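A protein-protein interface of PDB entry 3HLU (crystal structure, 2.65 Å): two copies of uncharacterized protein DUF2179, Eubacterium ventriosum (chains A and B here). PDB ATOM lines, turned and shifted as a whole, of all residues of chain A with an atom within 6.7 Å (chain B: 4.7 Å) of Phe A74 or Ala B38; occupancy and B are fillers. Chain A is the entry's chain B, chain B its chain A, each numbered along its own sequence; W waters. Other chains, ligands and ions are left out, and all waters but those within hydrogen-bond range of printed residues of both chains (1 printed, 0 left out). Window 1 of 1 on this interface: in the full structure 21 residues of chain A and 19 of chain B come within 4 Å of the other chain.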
ATOM      1  N   TYR A  12       3.396  25.386   1.704  1.00  0.00           N
ATOM      2  CA  TYR A  12       2.313  24.482   2.001  1.00  0.00           C
ATOM      3  C   TYR A  12       1.527  24.197   0.734  1.00  0.00           C
ATOM      4  O   TYR A  12       1.208  25.093  -0.039  1.00  0.00           O
ATOM      5  CB  TYR A  12       1.420  25.046   3.089  1.00  0.00           C
ATOM      6  CG  TYR A  12       2.192  25.608   4.255  1.00  0.00           C
ATOM      7  CD1 TYR A  12       2.514  26.951   4.306  1.00  0.00           C
ATOM      8  CD2 TYR A  12       2.594  24.796   5.317  1.00  0.00           C
ATOM      9  CE1 TYR A  12       3.210  27.479   5.375  1.00  0.00           C
ATOM     10  CE2 TYR A  12       3.296  25.320   6.398  1.00  0.00           C
ATOM     11  CZ  TYR A  12       3.599  26.667   6.415  1.00  0.00           C
ATOM     12  OH  TYR A  12       4.304  27.223   7.462  1.00  0.00           O
ATOM     13  N   ILE A  13       1.245  22.928   0.515  1.00  0.00           N
ATOM     14  CA  ILE A  13       0.489  22.523  -0.635  1.00  0.00           C
ATOM     15  C   ILE A  13      -0.798  21.887  -0.174  1.00  0.00           C
ATOM     16  O   ILE A  13      -0.784  20.911   0.567  1.00  0.00           O
ATOM     17  CB  ILE A  13       1.260  21.494  -1.432  1.00  0.00           C
ATOM     18  CG1 ILE A  13       2.600  22.080  -1.884  1.00  0.00           C
ATOM     19  CG2 ILE A  13       0.401  20.939  -2.584  1.00  0.00           C
ATOM     20  CD1 ILE A  13       3.490  21.047  -2.547  1.00  0.00           C
ATOM     21  N   VAL A  14      -1.907  22.462  -0.628  1.00  0.00           N
ATOM     22  CA  VAL A  14      -3.236  21.965  -0.324  1.00  0.00           C
ATOM     23  C   VAL A  14      -3.786  21.171  -1.484  1.00  0.00           C
ATOM     24  O   VAL A  14      -3.835  21.663  -2.597  1.00  0.00           O
ATOM     25  CB  VAL A  14      -4.192  23.127  -0.109  1.00  0.00           C
ATOM     26  CG1 VAL A  14      -5.602  22.610   0.239  1.00  0.00           C
ATOM     27  CG2 VAL A  14      -3.639  24.066   0.950  1.00  0.00           C
ATOM     28  N   SER A  15      -4.232  19.950  -1.220  1.00  0.00           N
ATOM     29  CA  SER A  15      -4.767  19.117  -2.278  1.00  0.00           C
ATOM     30  C   SER A  15      -5.462  17.858  -1.776  1.00  0.00           C
ATOM     31  O   SER A  15      -4.997  17.197  -0.853  1.00  0.00           O
ATOM     32  CB  SER A  15      -3.653  18.737  -3.244  1.00  0.00           C
ATOM     33  OG  SER A  15      -3.989  17.592  -3.997  1.00  0.00           O
ATOM     34  N   ARG A  63       5.091  22.814  -9.205  1.00  0.00           N
ATOM     35  CA  ARG A  63       3.931  23.369  -9.847  1.00  0.00           C
ATOM     36  C   ARG A  63       3.497  22.488 -11.008  1.00  0.00           C
ATOM     37  O   ARG A  63       2.316  22.211 -11.174  1.00  0.00           O
ATOM     38  CB  ARG A  63       4.268  24.759 -10.365  1.00  0.00           C
ATOM     39  CG  ARG A  63       3.163  25.739 -10.166  1.00  0.00           C
ATOM     40  CD  ARG A  63       2.951  26.585 -11.381  1.00  0.00           C
ATOM     41  NE  ARG A  63       1.832  27.496 -11.160  1.00  0.00           N
ATOM     42  CZ  ARG A  63       1.960  28.817 -11.034  1.00  0.00           C
ATOM     43  NH1 ARG A  63       3.169  29.368 -11.132  1.00  0.00           N
ATOM     44  NH2 ARG A  63       0.888  29.585 -10.818  1.00  0.00           N
ATOM     45  N   LEU A  66       1.897  19.446 -10.029  1.00  0.00           N
ATOM     46  CA  LEU A  66       0.513  19.671  -9.635  1.00  0.00           C
ATOM     47  C   LEU A  66      -0.432  19.595 -10.829  1.00  0.00           C
ATOM     48  O   LEU A  66      -1.479  18.944 -10.767  1.00  0.00           O
ATOM     49  CB  LEU A  66       0.352  21.027  -8.961  1.00  0.00           C
ATOM     50  CG  LEU A  66       1.045  21.229  -7.625  1.00  0.00           C
ATOM     51  CD1 LEU A  66       0.502  22.488  -6.927  1.00  0.00           C
ATOM     52  CD2 LEU A  66       0.866  19.967  -6.789  1.00  0.00           C
ATOM     53  N   ASP A  70      -3.458  17.287  -9.699  1.00  0.00           N
ATOM     54  CA  ASP A  70      -4.611  17.995  -9.148  1.00  0.00           C
ATOM     55  C   ASP A  70      -4.589  19.443  -9.629  1.00  0.00           C
ATOM     56  O   ASP A  70      -3.901  20.283  -9.061  1.00  0.00           O
ATOM     57  CB  ASP A  70      -4.620  17.918  -7.611  1.00  0.00           C
ATOM     58  CG  ASP A  70      -5.835  18.609  -6.986  1.00  0.00           C
ATOM     59  OD1 ASP A  70      -6.009  18.529  -5.739  1.00  0.00           O
ATOM     60  OD2 ASP A  70      -6.616  19.240  -7.736  1.00  0.00           O
ATOM     61  N   PRO A  71      -5.338  19.730 -10.707  1.00  0.00           N
ATOM     62  CA  PRO A  71      -5.442  21.087 -11.252  1.00  0.00           C
ATOM     63  C   PRO A  71      -5.982  22.050 -10.219  1.00  0.00           C
ATOM     64  O   PRO A  71      -5.826  23.264 -10.358  1.00  0.00           O
ATOM     65  CB  PRO A  71      -6.463  20.916 -12.375  1.00  0.00           C
ATOM     66  CG  PRO A  71      -6.325  19.508 -12.795  1.00  0.00           C
ATOM     67  CD  PRO A  71      -6.032  18.744 -11.541  1.00  0.00           C
ATOM     68  N   ASP A  72      -6.619  21.512  -9.185  1.00  0.00           N
ATOM     69  CA  ASP A  72      -7.202  22.356  -8.142  1.00  0.00           C
ATOM     70  C   ASP A  72      -6.309  22.550  -6.924  1.00  0.00           C
ATOM     71  O   ASP A  72      -6.627  23.340  -6.039  1.00  0.00           O
ATOM     72  CB  ASP A  72      -8.566  21.828  -7.722  1.00  0.00           C
ATOM     73  CG  ASP A  72      -9.578  21.898  -8.848  1.00  0.00           C
ATOM     74  OD1 ASP A  72      -9.731  22.996  -9.460  1.00  0.00           O
ATOM     75  OD2 ASP A  72     -10.198  20.841  -9.130  1.00  0.00           O
ATOM     76  N   ALA A  73      -5.195  21.836  -6.880  1.00  0.00           N
ATOM     77  CA  ALA A  73      -4.218  22.055  -5.833  1.00  0.00           C
ATOM     78  C   ALA A  73      -3.654  23.466  -5.939  1.00  0.00           C
ATOM     79  O   ALA A  73      -3.635  24.079  -7.009  1.00  0.00           O
ATOM     80  CB  ALA A  73      -3.099  21.022  -5.921  1.00  0.00           C
ATOM     81  N   PHE A  74      -3.203  23.978  -4.806  1.00  0.00           N
ATOM     82  CA  PHE A  74      -2.505  25.245  -4.771  1.00  0.00           C
ATOM     83  C   PHE A  74      -1.535  25.255  -3.590  1.00  0.00           C
ATOM     84  O   PHE A  74      -1.603  24.416  -2.690  1.00  0.00           O
ATOM     85  CB  PHE A  74      -3.494  26.386  -4.639  1.00  0.00           C
ATOM     86  CG  PHE A  74      -4.324  26.300  -3.406  1.00  0.00           C
ATOM     87  CD1 PHE A  74      -5.478  25.535  -3.386  1.00  0.00           C
ATOM     88  CD2 PHE A  74      -3.934  26.949  -2.242  1.00  0.00           C
ATOM     89  CE1 PHE A  74      -6.237  25.448  -2.240  1.00  0.00           C
ATOM     90  CE2 PHE A  74      -4.697  26.856  -1.090  1.00  0.00           C
ATOM     91  CZ  PHE A  74      -5.852  26.115  -1.095  1.00  0.00           C
ATOM     92  N   MET A  75      -0.632  26.221  -3.611  1.00  0.00           N
ATOM     93  CA  MET A  75       0.438  26.272  -2.648  1.00  0.00           C
ATOM     94  C   MET A  75       0.472  27.608  -1.983  1.00  0.00           C
ATOM     95  O   MET A  75       0.232  28.634  -2.614  1.00  0.00           O
ATOM     96  CB  MET A  75       1.779  26.080  -3.344  1.00  0.00           C
ATOM     97  CG  MET A  75       1.860  24.860  -4.253  1.00  0.00           C
ATOM     98  SD  MET A  75       3.474  24.933  -5.386  1.00  0.00           S
ATOM     99  CE  MET A  75       4.675  23.909  -4.252  1.00  0.00           C
ATOM    100  N   ILE A  76       0.809  27.591  -0.704  1.00  0.00           N
ATOM    101  CA  ILE A  76       1.054  28.812   0.017  1.00  0.00           C
ATOM    102  C   ILE A  76       2.533  28.998   0.219  1.00  0.00           C
ATOM    103  O   ILE A  76       3.182  28.216   0.898  1.00  0.00           O
ATOM    104  CB  ILE A  76       0.373  28.782   1.360  1.00  0.00           C
ATOM    105  CG1 ILE A  76      -1.136  28.701   1.157  1.00  0.00           C
ATOM    106  CG2 ILE A  76       0.758  30.006   2.155  1.00  0.00           C
ATOM    107  CD1 ILE A  76      -1.862  28.261   2.376  1.00  0.00           C
ATOM    108  N   VAL A  77       3.071  30.043  -0.389  1.00  0.00           N
ATOM    109  CA  VAL A  77       4.493  30.322  -0.289  1.00  0.00           C
ATOM    110  C   VAL A  77       4.807  31.326   0.824  1.00  0.00           C
ATOM    111  O   VAL A  77       4.617  32.543   0.651  1.00  0.00           O
ATOM    112  CB  VAL A  77       5.042  30.873  -1.607  1.00  0.00           C
ATOM    113  CG1 VAL A  77       6.516  31.213  -1.440  1.00  0.00           C
ATOM    114  CG2 VAL A  77       4.814  29.870  -2.746  1.00  0.00           C
ATOM    115  N   VAL B  14      -7.905  28.739   5.140  1.00  0.00           N
ATOM    116  CA  VAL B  14      -8.459  28.281   3.881  1.00  0.00           C
ATOM    117  C   VAL B  14      -9.956  28.098   3.982  1.00  0.00           C
ATOM    118  O   VAL B  14     -10.424  27.253   4.725  1.00  0.00           O
ATOM    119  CB  VAL B  14      -7.898  26.920   3.495  1.00  0.00           C
ATOM    120  CG1 VAL B  14      -8.440  26.510   2.130  1.00  0.00           C
ATOM    121  CG2 VAL B  14      -6.384  26.939   3.515  1.00  0.00           C
ATOM    122  N   LEU B  36      -4.119  37.221   0.991  1.00  0.00           N
ATOM    123  CA  LEU B  36      -3.066  36.614   0.188  1.00  0.00           C
ATOM    124  C   LEU B  36      -3.568  35.713  -0.948  1.00  0.00           C
ATOM    125  O   LEU B  36      -4.648  35.115  -0.883  1.00  0.00           O
ATOM    126  CB  LEU B  36      -2.145  35.816   1.107  1.00  0.00           C
ATOM    127  CG  LEU B  36      -1.079  34.970   0.420  1.00  0.00           C
ATOM    128  CD1 LEU B  36      -0.223  35.850  -0.484  1.00  0.00           C
ATOM    129  CD2 LEU B  36      -0.206  34.235   1.446  1.00  0.00           C
ATOM    130  N   GLN B  37      -2.770  35.626  -2.003  1.00  0.00           N
ATOM    131  CA  GLN B  37      -3.145  34.853  -3.181  1.00  0.00           C
ATOM    132  C   GLN B  37      -2.210  33.655  -3.360  1.00  0.00           C
ATOM    133  O   GLN B  37      -0.992  33.805  -3.379  1.00  0.00           O
ATOM    134  CB  GLN B  37      -3.138  35.749  -4.422  1.00  0.00           C
ATOM    135  CG  GLN B  37      -3.879  35.169  -5.609  1.00  0.00           C
ATOM    136  CD  GLN B  37      -4.588  36.245  -6.400  1.00  0.00           C
ATOM    137  OE1 GLN B  37      -4.128  36.651  -7.478  1.00  0.00           O
ATOM    138  NE2 GLN B  37      -5.709  36.737  -5.857  1.00  0.00           N
ATOM    139  N   ALA B  38      -2.791  32.465  -3.484  1.00  0.00           N
ATOM    140  CA  ALA B  38      -2.005  31.237  -3.524  1.00  0.00           C
ATOM    141  C   ALA B  38      -1.426  30.959  -4.918  1.00  0.00           C
ATOM    142  O   ALA B  38      -1.925  31.465  -5.919  1.00  0.00           O
ATOM    143  CB  ALA B  38      -2.846  30.054  -3.039  1.00  0.00           C
ATOM    144  N   VAL B  39      -0.360  30.174  -4.978  1.00  0.00           N
ATOM    145  CA  VAL B  39       0.175  29.763  -6.256  1.00  0.00           C
ATOM    146  C   VAL B  39      -0.533  28.472  -6.571  1.00  0.00           C
ATOM    147  O   VAL B  39      -0.243  27.444  -5.960  1.00  0.00           O
ATOM    148  CB  VAL B  39       1.716  29.549  -6.183  1.00  0.00           C
ATOM    149  CG1 VAL B  39       2.261  28.888  -7.460  1.00  0.00           C
ATOM    150  CG2 VAL B  39       2.432  30.877  -5.900  1.00  0.00           C
ATOM    151  N   GLY B  40      -1.490  28.522  -7.490  1.00  0.00           N
ATOM    152  CA  GLY B  40      -2.175  27.306  -7.904  1.00  0.00           C
ATOM    153  C   GLY B  40      -1.379  26.506  -8.920  1.00  0.00           C
ATOM    154  O   GLY B  40      -0.333  26.945  -9.380  1.00  0.00           O
ATOM    155  N   ALA B  41      -1.861  25.326  -9.274  1.00  0.00           N
ATOM    156  CA  ALA B  41      -1.257  24.556 -10.363  1.00  0.00           C
ATOM    157  C   ALA B  41      -1.159  25.365 -11.677  1.00  0.00           C
ATOM    158  O   ALA B  41      -0.176  25.257 -12.407  1.00  0.00           O
ATOM    159  CB  ALA B  41      -2.032  23.277 -10.581  1.00  0.00           C
ATOM    160  N   THR B  47      -6.907  31.246  -6.169  1.00  0.00           N
ATOM    161  CA  THR B  47      -7.510  30.882  -4.904  1.00  0.00           C
ATOM    162  C   THR B  47      -6.883  31.821  -3.868  1.00  0.00           C
ATOM    163  O   THR B  47      -5.688  32.122  -3.909  1.00  0.00           O
ATOM    164  CB  THR B  47      -7.299  29.378  -4.605  1.00  0.00           C
ATOM    165  OG1 THR B  47      -7.870  29.026  -3.336  1.00  0.00           O
ATOM    166  CG2 THR B  47      -5.823  29.043  -4.629  1.00  0.00           C
ATOM    167  N   VAL B  49      -6.266  33.211   0.104  1.00  0.00           N
ATOM    168  CA  VAL B  49      -6.091  32.737   1.448  1.00  0.00           C
ATOM    169  C   VAL B  49      -6.108  33.950   2.378  1.00  0.00           C
ATOM    170  O   VAL B  49      -5.639  35.012   2.000  1.00  0.00           O
ATOM    171  CB  VAL B  49      -4.762  31.946   1.514  1.00  0.00           C
ATOM    172  CG1 VAL B  49      -4.107  32.024   2.883  1.00  0.00           C
ATOM    173  CG2 VAL B  49      -4.990  30.516   1.065  1.00  0.00           C
HETATM  174  O   HOH W   1      -4.678  25.851  -9.887  1.00  0.00           O
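The backbone NH (N) of Met A75 lies within hydrogen-bond range of the backbone carbonyl oxygen (O) of Val B39 (2.7 Å). O of Gly B40 lies within hydrogen-bond range of NE of Arg A63 (2.9 Å). The backbone carbonyl oxygen of Ala B41 lies within hydrogen-bond range of the guanidinium group of Arg A63, at 3.3 Å. N of Ala B41 is in hydrogen-bond range of O of Ala A73 (3.1 Å).
N of Ala B38 sits at hydrogen-bond distance from O of Thr B47 (2.9 Å). O of Phe A74 lies within hydrogen-bond range of N of Val A14. OG of Ser A15 lies within hydrogen-bond range of OD1 of Asp A70 (2.8 Å). The side-chain carboxylate (OD2) of Asp A70 lies within hydrogen-bond range of the backbone NH (N) of Asp A72, at 2.7 Å. The backbone NH (N) of Ala A73 lies within hydrogen-bond range of the side-chain carboxylate (OD2) of Asp A70.
Arg A63 touches Val B39 (CZ to CG1, 3.6 Å). Leu A66 touches Ala B41. O of Asp A70 touches CB of Ala B41 (3.8 Å). O of Pro A71 touches CB of Ala B41, 3.8 Å away. CA of Gly B40 touches O of Ala A73 (3.7 Å). Ala B38 touches Phe A74. Val B39 touches Phe A74. CB of Phe A74 touches CA of Gly B40, 3.6 Å away. Thr B47 touches Phe A74. CB of Ala B38 touches O of Met A75, 3.4 Å away.
Val A77 touches none of the printed residues of chain B. Ala B38 touches just these residues of chain A: Phe A74 and Met A75. Printed residues of chain A within 4 Å of Val B39: Arg A63 (3.6 Å), Phe A74 (3.4 Å) and Met A75 (2.7 Å). Of the printed residues of chain A, Gly B40 touches Arg A63, Ala A73 and Phe A74. The nearest residue of chain B that does not touch Phe A74 is Val B14 (4.2 Å). The nearest residue of chain A that does not touch Ala B38 is Ile A76 (4.7 Å). The nearest printed residue of chain B that does not touch Pro A71 is Gly B40 (5.7 Å).
Printed residues of chain B that touch a printed residue of chain A: Ala B38, Val B39, Gly B40, Ala B41 and Thr B47. Hydrophobic or aromatic side chains of chain B within 4 Å of the printed part of chain A: Ala B38, Val B39 and Ala B41. Of the 14 printed residues of chain A, 7 touch a printed residue of chain B. Hydrophobic or aromatic side chains of chain A within 4 Å of the printed part of chain B: Leu A66, Phe A74 and Met A75.
Position printed for both chains: 14. Of the 14 pairs that touch across the chains among the printed residues, none has its exchanged pair printed and touching as well.
Water W1 bridges O of Pro A71 (2.9 Å) and N of Ala B41 (2.9 Å).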
